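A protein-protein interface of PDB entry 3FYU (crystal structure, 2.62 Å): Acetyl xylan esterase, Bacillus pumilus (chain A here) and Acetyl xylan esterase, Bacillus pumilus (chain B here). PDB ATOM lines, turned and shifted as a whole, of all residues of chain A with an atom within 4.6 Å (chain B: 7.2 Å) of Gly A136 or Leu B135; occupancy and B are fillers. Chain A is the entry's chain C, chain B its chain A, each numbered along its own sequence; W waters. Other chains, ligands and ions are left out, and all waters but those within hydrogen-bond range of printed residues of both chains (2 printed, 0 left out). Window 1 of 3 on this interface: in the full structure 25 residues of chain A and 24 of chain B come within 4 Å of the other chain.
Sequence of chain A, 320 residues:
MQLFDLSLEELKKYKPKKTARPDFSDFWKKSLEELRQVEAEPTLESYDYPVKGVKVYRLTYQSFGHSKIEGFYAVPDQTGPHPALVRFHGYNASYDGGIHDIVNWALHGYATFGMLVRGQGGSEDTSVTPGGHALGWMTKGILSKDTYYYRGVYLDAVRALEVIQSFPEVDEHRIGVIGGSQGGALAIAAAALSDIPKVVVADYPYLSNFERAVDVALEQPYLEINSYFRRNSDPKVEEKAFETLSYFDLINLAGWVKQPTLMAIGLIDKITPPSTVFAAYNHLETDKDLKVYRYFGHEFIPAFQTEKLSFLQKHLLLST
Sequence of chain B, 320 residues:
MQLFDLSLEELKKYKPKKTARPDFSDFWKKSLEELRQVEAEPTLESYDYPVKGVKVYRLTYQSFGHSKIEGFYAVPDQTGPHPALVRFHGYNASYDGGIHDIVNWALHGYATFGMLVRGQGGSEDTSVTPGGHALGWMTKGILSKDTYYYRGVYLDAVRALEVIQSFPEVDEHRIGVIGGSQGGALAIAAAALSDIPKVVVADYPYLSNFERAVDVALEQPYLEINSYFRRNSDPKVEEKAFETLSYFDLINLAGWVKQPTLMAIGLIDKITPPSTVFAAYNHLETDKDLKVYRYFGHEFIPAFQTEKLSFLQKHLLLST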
ATOM      1  N   TYR A  91      -6.880 -16.752  19.746  1.00  0.00           N
ATOM      2  CA  TYR A  91      -6.419 -15.514  20.350  1.00  0.00           C
ATOM      3  C   TYR A  91      -7.513 -14.808  21.168  1.00  0.00           C
ATOM      4  O   TYR A  91      -8.536 -14.366  20.622  1.00  0.00           O
ATOM      5  CB  TYR A  91      -5.923 -14.582  19.238  1.00  0.00           C
ATOM      6  CG  TYR A  91      -5.220 -13.331  19.711  1.00  0.00           C
ATOM      7  CD1 TYR A  91      -3.862 -13.351  20.002  1.00  0.00           C
ATOM      8  CD2 TYR A  91      -5.906 -12.120  19.845  1.00  0.00           C
ATOM      9  CE1 TYR A  91      -3.193 -12.200  20.413  1.00  0.00           C
ATOM     10  CE2 TYR A  91      -5.249 -10.963  20.253  1.00  0.00           C
ATOM     11  CZ  TYR A  91      -3.888 -11.015  20.537  1.00  0.00           C
ATOM     12  OH  TYR A  91      -3.215  -9.894  20.962  1.00  0.00           O
ATOM     13  N   ASN A  92      -7.297 -14.708  22.478  1.00  0.00           N
ATOM     14  CA  ASN A  92      -8.242 -14.022  23.358  1.00  0.00           C
ATOM     15  C   ASN A  92      -9.630 -14.632  23.230  1.00  0.00           C
ATOM     16  O   ASN A  92     -10.631 -13.984  23.543  1.00  0.00           O
ATOM     17  CB  ASN A  92      -8.276 -12.528  22.984  1.00  0.00           C
ATOM     18  CG  ASN A  92      -9.205 -11.704  23.865  1.00  0.00           C
ATOM     19  OD1 ASN A  92      -9.083 -11.696  25.090  1.00  0.00           O
ATOM     20  ND2 ASN A  92     -10.127 -10.992  23.237  1.00  0.00           N
ATOM     21  N   HIS A 133       4.294  -1.389  23.505  1.00  0.00           N
ATOM     22  CA  HIS A 133       3.746  -2.215  22.449  1.00  0.00           C
ATOM     23  C   HIS A 133       2.258  -1.916  22.298  1.00  0.00           C
ATOM     24  O   HIS A 133       1.635  -1.323  23.186  1.00  0.00           O
ATOM     25  CB  HIS A 133       3.997  -3.704  22.746  1.00  0.00           C
ATOM     26  CG  HIS A 133       3.288  -4.229  23.957  1.00  0.00           C
ATOM     27  ND1 HIS A 133       1.953  -4.569  23.952  1.00  0.00           N
ATOM     28  CD2 HIS A 133       3.745  -4.527  25.196  1.00  0.00           C
ATOM     29  CE1 HIS A 133       1.620  -5.060  25.132  1.00  0.00           C
ATOM     30  NE2 HIS A 133       2.689  -5.046  25.905  1.00  0.00           N
ATOM     31  N   ALA A 134       1.696  -2.311  21.161  1.00  0.00           N
ATOM     32  CA  ALA A 134       0.280  -2.079  20.890  1.00  0.00           C
ATOM     33  C   ALA A 134      -0.605  -2.891  21.826  1.00  0.00           C
ATOM     34  O   ALA A 134      -0.182  -3.901  22.383  1.00  0.00           O
ATOM     35  CB  ALA A 134      -0.034  -2.428  19.442  1.00  0.00           C
ATOM     36  N   LEU A 135      -1.833  -2.426  22.005  1.00  0.00           N
ATOM     37  CA  LEU A 135      -2.801  -3.101  22.860  1.00  0.00           C
ATOM     38  C   LEU A 135      -2.899  -4.556  22.396  1.00  0.00           C
ATOM     39  O   LEU A 135      -3.237  -4.825  21.239  1.00  0.00           O
ATOM     40  CB  LEU A 135      -4.156  -2.414  22.707  1.00  0.00           C
ATOM     41  CG  LEU A 135      -5.263  -2.537  23.756  1.00  0.00           C
ATOM     42  CD1 LEU A 135      -6.537  -1.956  23.164  1.00  0.00           C
ATOM     43  CD2 LEU A 135      -5.502  -3.972  24.126  1.00  0.00           C
ATOM     44  N   GLY A 136      -2.594  -5.491  23.294  1.00  0.00           N
ATOM     45  CA  GLY A 136      -2.662  -6.895  22.936  1.00  0.00           C
ATOM     46  C   GLY A 136      -1.360  -7.646  23.192  1.00  0.00           C
ATOM     47  O   GLY A 136      -0.417  -7.089  23.769  1.00  0.00           O
ATOM     48  N   TRP A 137      -1.304  -8.907  22.760  1.00  0.00           N
ATOM     49  CA  TRP A 137      -0.120  -9.740  22.951  1.00  0.00           C
ATOM     50  C   TRP A 137       0.730  -9.818  21.688  1.00  0.00           C
ATOM     51  O   TRP A 137       1.910 -10.135  21.751  1.00  0.00           O
ATOM     52  CB  TRP A 137      -0.530 -11.158  23.343  1.00  0.00           C
ATOM     53  CG  TRP A 137      -1.211 -11.260  24.661  1.00  0.00           C
ATOM     54  CD1 TRP A 137      -0.613 -11.358  25.883  1.00  0.00           C
ATOM     55  CD2 TRP A 137      -2.629 -11.299  24.900  1.00  0.00           C
ATOM     56  NE1 TRP A 137      -1.565 -11.461  26.870  1.00  0.00           N
ATOM     57  CE2 TRP A 137      -2.810 -11.428  26.294  1.00  0.00           C
ATOM     58  CE3 TRP A 137      -3.761 -11.242  24.071  1.00  0.00           C
ATOM     59  CZ2 TRP A 137      -4.079 -11.502  26.879  1.00  0.00           C
ATOM     60  CZ3 TRP A 137      -5.018 -11.317  24.652  1.00  0.00           C
ATOM     61  CH2 TRP A 137      -5.166 -11.446  26.041  1.00  0.00           C
ATOM     62  N   MET A 138       0.130  -9.520  20.542  1.00  0.00           N
ATOM     63  CA  MET A 138       0.843  -9.601  19.273  1.00  0.00           C
ATOM     64  C   MET A 138       2.201  -8.897  19.189  1.00  0.00           C
ATOM     65  O   MET A 138       3.106  -9.367  18.495  1.00  0.00           O
ATOM     66  CB  MET A 138      -0.046  -9.098  18.130  1.00  0.00           C
ATOM     67  CG  MET A 138      -1.206 -10.026  17.802  1.00  0.00           C
ATOM     68  SD  MET A 138      -0.662 -11.731  17.587  1.00  0.00           S
ATOM     69  CE  MET A 138       0.271 -11.606  16.034  1.00  0.00           C
ATOM     70  N   GLU A 224      -2.663  -5.560  14.989  1.00  0.00           N
ATOM     71  CA  GLU A 224      -2.038  -5.075  16.214  1.00  0.00           C
ATOM     72  C   GLU A 224      -0.626  -4.634  15.847  1.00  0.00           C
ATOM     73  O   GLU A 224      -0.076  -3.688  16.412  1.00  0.00           O
ATOM     74  CB  GLU A 224      -1.988  -6.175  17.282  1.00  0.00           C
ATOM     75  CG  GLU A 224      -3.182  -6.186  18.214  1.00  0.00           C
ATOM     76  CD  GLU A 224      -3.128  -7.320  19.231  1.00  0.00           C
ATOM     77  OE1 GLU A 224      -2.044  -7.571  19.795  1.00  0.00           O
ATOM     78  OE2 GLU A 224      -4.174  -7.958  19.485  1.00  0.00           O
ATOM     79  N   TYR B  91      -4.448   5.857  27.647  1.00  0.00           N
ATOM     80  CA  TYR B  91      -4.396   4.417  27.469  1.00  0.00           C
ATOM     81  C   TYR B  91      -4.125   4.037  26.012  1.00  0.00           C
ATOM     82  O   TYR B  91      -4.931   4.345  25.123  1.00  0.00           O
ATOM     83  CB  TYR B  91      -5.722   3.818  27.906  1.00  0.00           C
ATOM     84  CG  TYR B  91      -5.745   2.309  27.984  1.00  0.00           C
ATOM     85  CD1 TYR B  91      -5.294   1.647  29.122  1.00  0.00           C
ATOM     86  CD2 TYR B  91      -6.256   1.540  26.933  1.00  0.00           C
ATOM     87  CE1 TYR B  91      -5.356   0.261  29.219  1.00  0.00           C
ATOM     88  CE2 TYR B  91      -6.316   0.148  27.028  1.00  0.00           C
ATOM     89  CZ  TYR B  91      -5.865  -0.475  28.174  1.00  0.00           C
ATOM     90  OH  TYR B  91      -5.899  -1.839  28.288  1.00  0.00           O
ATOM     91  N   ASN B  92      -2.988   3.379  25.777  1.00  0.00           N
ATOM     92  CA  ASN B  92      -2.618   2.930  24.439  1.00  0.00           C
ATOM     93  C   ASN B  92      -2.627   4.090  23.442  1.00  0.00           C
ATOM     94  O   ASN B  92      -2.725   3.889  22.232  1.00  0.00           O
ATOM     95  CB  ASN B  92      -3.604   1.840  24.000  1.00  0.00           C
ATOM     96  CG  ASN B  92      -3.270   1.248  22.646  1.00  0.00           C
ATOM     97  OD1 ASN B  92      -2.180   0.721  22.436  1.00  0.00           O
ATOM     98  ND2 ASN B  92      -4.213   1.325  21.724  1.00  0.00           N
ATOM     99  N   GLY B 119       4.795  -0.906  29.211  1.00  0.00           N
ATOM    100  CA  GLY B 119       4.301  -1.702  28.103  1.00  0.00           C
ATOM    101  C   GLY B 119       3.402  -1.008  27.097  1.00  0.00           C
ATOM    102  O   GLY B 119       3.027  -1.602  26.081  1.00  0.00           O
ATOM    103  N   HIS B 133      -6.352 -13.032  31.320  1.00  0.00           N
ATOM    104  CA  HIS B 133      -7.008 -11.750  31.439  1.00  0.00           C
ATOM    105  C   HIS B 133      -7.473 -11.304  30.062  1.00  0.00           C
ATOM    106  O   HIS B 133      -7.042 -11.844  29.039  1.00  0.00           O
ATOM    107  CB  HIS B 133      -6.069 -10.713  32.083  1.00  0.00           C
ATOM    108  CG  HIS B 133      -4.851 -10.383  31.272  1.00  0.00           C
ATOM    109  ND1 HIS B 133      -4.885  -9.537  30.187  1.00  0.00           N
ATOM    110  CD2 HIS B 133      -3.556 -10.751  31.421  1.00  0.00           C
ATOM    111  CE1 HIS B 133      -3.663  -9.393  29.704  1.00  0.00           C
ATOM    112  NE2 HIS B 133      -2.839 -10.119  30.435  1.00  0.00           N
ATOM    113  N   ALA B 134      -8.375 -10.334  30.037  1.00  0.00           N
ATOM    114  CA  ALA B 134      -8.890  -9.841  28.779  1.00  0.00           C
ATOM    115  C   ALA B 134      -7.807  -9.134  27.973  1.00  0.00           C
ATOM    116  O   ALA B 134      -6.799  -8.701  28.518  1.00  0.00           O
ATOM    117  CB  ALA B 134     -10.044  -8.900  29.044  1.00  0.00           C
ATOM    118  N   LEU B 135      -8.025  -9.038  26.667  1.00  0.00           N
ATOM    119  CA  LEU B 135      -7.104  -8.363  25.760  1.00  0.00           C
ATOM    120  C   LEU B 135      -6.893  -6.937  26.289  1.00  0.00           C
ATOM    121  O   LEU B 135      -7.856  -6.174  26.415  1.00  0.00           O
ATOM    122  CB  LEU B 135      -7.731  -8.307  24.377  1.00  0.00           C
ATOM    123  CG  LEU B 135      -6.886  -8.083  23.127  1.00  0.00           C
ATOM    124  CD1 LEU B 135      -7.840  -7.808  21.972  1.00  0.00           C
ATOM    125  CD2 LEU B 135      -5.947  -6.925  23.306  1.00  0.00           C
ATOM    126  N   GLY B 136      -5.645  -6.584  26.603  1.00  0.00           N
ATOM    127  CA  GLY B 136      -5.364  -5.257  27.118  1.00  0.00           C
ATOM    128  C   GLY B 136      -4.667  -5.261  28.469  1.00  0.00           C
ATOM    129  O   GLY B 136      -4.316  -6.319  28.998  1.00  0.00           O
ATOM    130  N   TRP B 137      -4.472  -4.076  29.039  1.00  0.00           N
ATOM    131  CA  TRP B 137      -3.801  -3.953  30.324  1.00  0.00           C
ATOM    132  C   TRP B 137      -4.759  -3.856  31.496  1.00  0.00           C
ATOM    133  O   TRP B 137      -4.393  -4.175  32.631  1.00  0.00           O
ATOM    134  CB  TRP B 137      -2.907  -2.718  30.323  1.00  0.00           C
ATOM    135  CG  TRP B 137      -1.753  -2.808  29.376  1.00  0.00           C
ATOM    136  CD1 TRP B 137      -0.559  -3.450  29.582  1.00  0.00           C
ATOM    137  CD2 TRP B 137      -1.684  -2.244  28.065  1.00  0.00           C
ATOM    138  NE1 TRP B 137       0.246  -3.316  28.475  1.00  0.00           N
ATOM    139  CE2 TRP B 137      -0.419  -2.579  27.530  1.00  0.00           C
ATOM    140  CE3 TRP B 137      -2.567  -1.491  27.288  1.00  0.00           C
ATOM    141  CZ2 TRP B 137      -0.019  -2.181  26.250  1.00  0.00           C
ATOM    142  CZ3 TRP B 137      -2.172  -1.096  26.016  1.00  0.00           C
ATOM    143  CH2 TRP B 137      -0.912  -1.441  25.511  1.00  0.00           C
ATOM    144  N   MET B 138      -5.985  -3.427  31.213  1.00  0.00           N
ATOM    145  CA  MET B 138      -6.995  -3.239  32.246  1.00  0.00           C
ATOM    146  C   MET B 138      -7.206  -4.365  33.238  1.00  0.00           C
ATOM    147  O   MET B 138      -7.523  -4.103  34.395  1.00  0.00           O
ATOM    148  CB  MET B 138      -8.337  -2.888  31.609  1.00  0.00           C
ATOM    149  CG  MET B 138      -8.371  -1.505  30.989  1.00  0.00           C
ATOM    150  SD  MET B 138      -7.767  -0.250  32.149  1.00  0.00           S
ATOM    151  CE  MET B 138      -9.063  -0.264  33.406  1.00  0.00           C
ATOM    152  N   THR B 139      -7.037  -5.612  32.807  1.00  0.00           N
ATOM    153  CA  THR B 139      -7.256  -6.732  33.715  1.00  0.00           C
ATOM    154  C   THR B 139      -6.025  -7.562  34.050  1.00  0.00           C
ATOM    155  O   THR B 139      -6.135  -8.595  34.703  1.00  0.00           O
ATOM    156  CB  THR B 139      -8.369  -7.668  33.189  1.00  0.00           C
ATOM    157  OG1 THR B 139      -8.021  -8.162  31.894  1.00  0.00           O
ATOM    158  CG2 THR B 139      -9.654  -6.915  33.072  1.00  0.00           C
ATOM    159  N   GLN B 220     -14.252   1.139  24.719  1.00  0.00           N
ATOM    160  CA  GLN B 220     -13.110   0.653  25.477  1.00  0.00           C
ATOM    161  C   GLN B 220     -12.534   1.876  26.202  1.00  0.00           C
ATOM    162  O   GLN B 220     -12.839   3.016  25.846  1.00  0.00           O
ATOM    163  CB  GLN B 220     -12.068   0.057  24.533  1.00  0.00           C
ATOM    164  CG  GLN B 220     -12.586  -1.083  23.692  1.00  0.00           C
ATOM    165  CD  GLN B 220     -13.133  -2.209  24.540  1.00  0.00           C
ATOM    166  OE1 GLN B 220     -12.444  -2.723  25.425  1.00  0.00           O
ATOM    167  NE2 GLN B 220     -14.378  -2.599  24.280  1.00  0.00           N
ATOM    168  N   PRO B 221     -11.652   1.660  27.186  1.00  0.00           N
ATOM    169  CA  PRO B 221     -11.147   0.372  27.664  1.00  0.00           C
ATOM    170  C   PRO B 221     -11.783  -0.164  28.947  1.00  0.00           C
ATOM    171  O   PRO B 221     -11.377  -1.217  29.445  1.00  0.00           O
ATOM    172  CB  PRO B 221      -9.644   0.632  27.842  1.00  0.00           C
ATOM    173  CG  PRO B 221      -9.462   2.181  27.616  1.00  0.00           C
ATOM    174  CD  PRO B 221     -10.844   2.755  27.735  1.00  0.00           C
ATOM    175  N   GLU B 224     -13.025  -3.656  29.014  1.00  0.00           N
ATOM    176  CA  GLU B 224     -12.078  -4.754  29.048  1.00  0.00           C
ATOM    177  C   GLU B 224     -12.424  -5.573  30.279  1.00  0.00           C
ATOM    178  O   GLU B 224     -12.282  -6.796  30.285  1.00  0.00           O
ATOM    179  CB  GLU B 224     -10.638  -4.231  29.152  1.00  0.00           C
ATOM    180  CG  GLU B 224      -9.991  -3.932  27.813  1.00  0.00           C
ATOM    181  CD  GLU B 224      -8.572  -3.419  27.945  1.00  0.00           C
ATOM    182  OE1 GLU B 224      -7.858  -3.854  28.875  1.00  0.00           O
ATOM    183  OE2 GLU B 224      -8.166  -2.595  27.106  1.00  0.00           O
ATOM    184  N   ILE B 225     -12.881  -4.886  31.323  1.00  0.00           N
ATOM    185  CA  ILE B 225     -13.261  -5.550  32.566  1.00  0.00           C
ATOM    186  C   ILE B 225     -14.434  -6.479  32.283  1.00  0.00           C
ATOM    187  O   ILE B 225     -14.437  -7.621  32.727  1.00  0.00           O
ATOM    188  CB  ILE B 225     -13.647  -4.521  33.652  1.00  0.00           C
ATOM    189  CG1 ILE B 225     -12.431  -3.660  33.981  1.00  0.00           C
ATOM    190  CG2 ILE B 225     -14.133  -5.226  34.904  1.00  0.00           C
ATOM    191  CD1 ILE B 225     -12.716  -2.522  34.930  1.00  0.00           C
ATOM    192  N   SER B 227     -15.210  -7.782  29.447  1.00  0.00           N
ATOM    193  CA  SER B 227     -14.692  -8.881  28.645  1.00  0.00           C
ATOM    194  C   SER B 227     -14.017  -9.910  29.533  1.00  0.00           C
ATOM    195  O   SER B 227     -14.084 -11.108  29.276  1.00  0.00           O
ATOM    196  CB  SER B 227     -13.688  -8.364  27.622  1.00  0.00           C
ATOM    197  OG  SER B 227     -14.291  -7.435  26.736  1.00  0.00           O
ATOM    198  N   TYR B 228     -13.358  -9.431  30.580  1.00  0.00           N
ATOM    199  CA  TYR B 228     -12.660 -10.312  31.508  1.00  0.00           C
ATOM    200  C   TYR B 228     -13.663 -11.228  32.218  1.00  0.00           C
ATOM    201  O   TYR B 228     -13.450 -12.450  32.302  1.00  0.00           O
ATOM    202  CB  TYR B 228     -11.864  -9.478  32.524  1.00  0.00           C
ATOM    203  CG  TYR B 228     -11.202 -10.287  33.603  1.00  0.00           C
ATOM    204  CD1 TYR B 228     -10.067 -11.049  33.341  1.00  0.00           C
ATOM    205  CD2 TYR B 228     -11.740 -10.336  34.880  1.00  0.00           C
ATOM    206  CE1 TYR B 228      -9.489 -11.846  34.334  1.00  0.00           C
ATOM    207  CE2 TYR B 228     -11.172 -11.127  35.868  1.00  0.00           C
ATOM    208  CZ  TYR B 228     -10.052 -11.878  35.591  1.00  0.00           C
ATOM    209  OH  TYR B 228      -9.518 -12.660  36.587  1.00  0.00           O
ATOM    210  N   ARG B 231     -15.023 -14.069  30.271  1.00  0.00           N
ATOM    211  CA  ARG B 231     -14.073 -15.167  30.147  1.00  0.00           C
ATOM    212  C   ARG B 231     -13.824 -15.920  31.442  1.00  0.00           C
ATOM    213  O   ARG B 231     -13.229 -16.988  31.428  1.00  0.00           O
ATOM    214  CB  ARG B 231     -12.756 -14.639  29.558  1.00  0.00           C
ATOM    215  CG  ARG B 231     -12.902 -14.190  28.104  1.00  0.00           C
ATOM    216  CD  ARG B 231     -11.724 -13.384  27.588  1.00  0.00           C
ATOM    217  NE  ARG B 231     -11.854 -13.113  26.155  1.00  0.00           N
ATOM    218  CZ  ARG B 231     -12.811 -12.366  25.604  1.00  0.00           C
ATOM    219  NH1 ARG B 231     -13.739 -11.791  26.361  1.00  0.00           N
ATOM    220  NH2 ARG B 231     -12.860 -12.215  24.286  1.00  0.00           N
HETATM  221  O   HOH W   1      -7.857 -13.600  26.731  1.00  0.00           O
HETATM  222  O   HOH W   2       2.234  -5.870  28.452  1.00  0.00           O
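Water W2 bridges NE2 of His A133 and NE1 of Trp B137.
Water W1 bridges the side-chain amide oxygen (OD1) of Asn A92 (2.8 Å) and the backbone carbonyl oxygen (O) of His B133 (3.0 Å).
Among the printed residues, pairs that only touch across the chains: His A133 with Trp B137 (3.5 Å), Ala A134 with Asn B92 (3.99 Å), Ala A134 with Trp B137 (3.97 Å), Leu A135 with Leu B135 (3.1 Å), Leu A135 with Gly B136 (3.3 Å), Leu A135 with Trp B137 (3.7 Å), Gly A136 with Leu B135 (3.3 Å), Trp A137 with His B133 (3.5 Å) and Trp A137 with Leu B135 (3.7 Å).
O of Asn A92 sits at hydrogen-bond distance from NH2 of Arg B231 (2.9 Å).
The backbone NH of His A133 is in hydrogen-bond range of the backbone carbonyl oxygen of Gly B119 (2.9 Å).
The backbone NH (N) of Leu B135 is in hydrogen-bond range of the side-chain amide oxygen (OD1) of Asn A92.
The backbone NH (N) of Leu A135 lies within hydrogen-bond range of the side-chain amide oxygen (OD1) of Asn B92.
O of Ser B227 sits at hydrogen-bond distance from NH1 of Arg B231, 3.0 Å away.
OH of Tyr B91 is in hydrogen-bond range of N of Trp B137.
A ring nitrogen (ND1) of His A133 sits close to the backbone carbonyl oxygen (O) of Gly A136, at 3.5 Å.
The backbone NH (N) of Trp A137 is in hydrogen-bond range of the side-chain carboxylate (OE1) of Glu A224 (3.3 Å).
ND1 of His B133 sits close to O of Gly B136, 3.5 Å away.
The backbone NH (N) of Trp B137 is in hydrogen-bond range of the side-chain carboxylate (OE1) of Glu B224 (3.4 Å).
Of the 9 printed residues of chain A, 6 touch a printed residue of chain B.
Printed residues of chain B that touch a printed residue of chain A: Asn B92, Gly B119, His B133, Leu B135, Gly B136, Trp B137 and Arg B231.
Hydrophobic or aromatic side chains of chain B that line the printed part of chain A: His B133, Leu B135 and Trp B137.
Among the printed residues, no Asp or Glu carboxylate lies within 4 Å of a Lys or Arg side-chain nitrogen of the other chain.
Of the printed residues of chain B, Ala A134 touches Asn B92 and Trp B137.
Of the printed residues of chain B, Gly A136 touches Leu B135 (3.3 Å).
Of the printed residues of chain A, His B133 touches Trp A137.
Leu B135 touches just these residues of chain A: Asn A92 (3.3 Å), Leu A135 (3.1 Å), Gly A136 (3.3 Å) and Trp A137 (3.7 Å).
The nearest residue of chain A that does not touch Leu B135 is Glu A224 (4.3 Å).
The nearest printed residue of chain A that does not touch His B133 is Asn A92 (4.4 Å).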
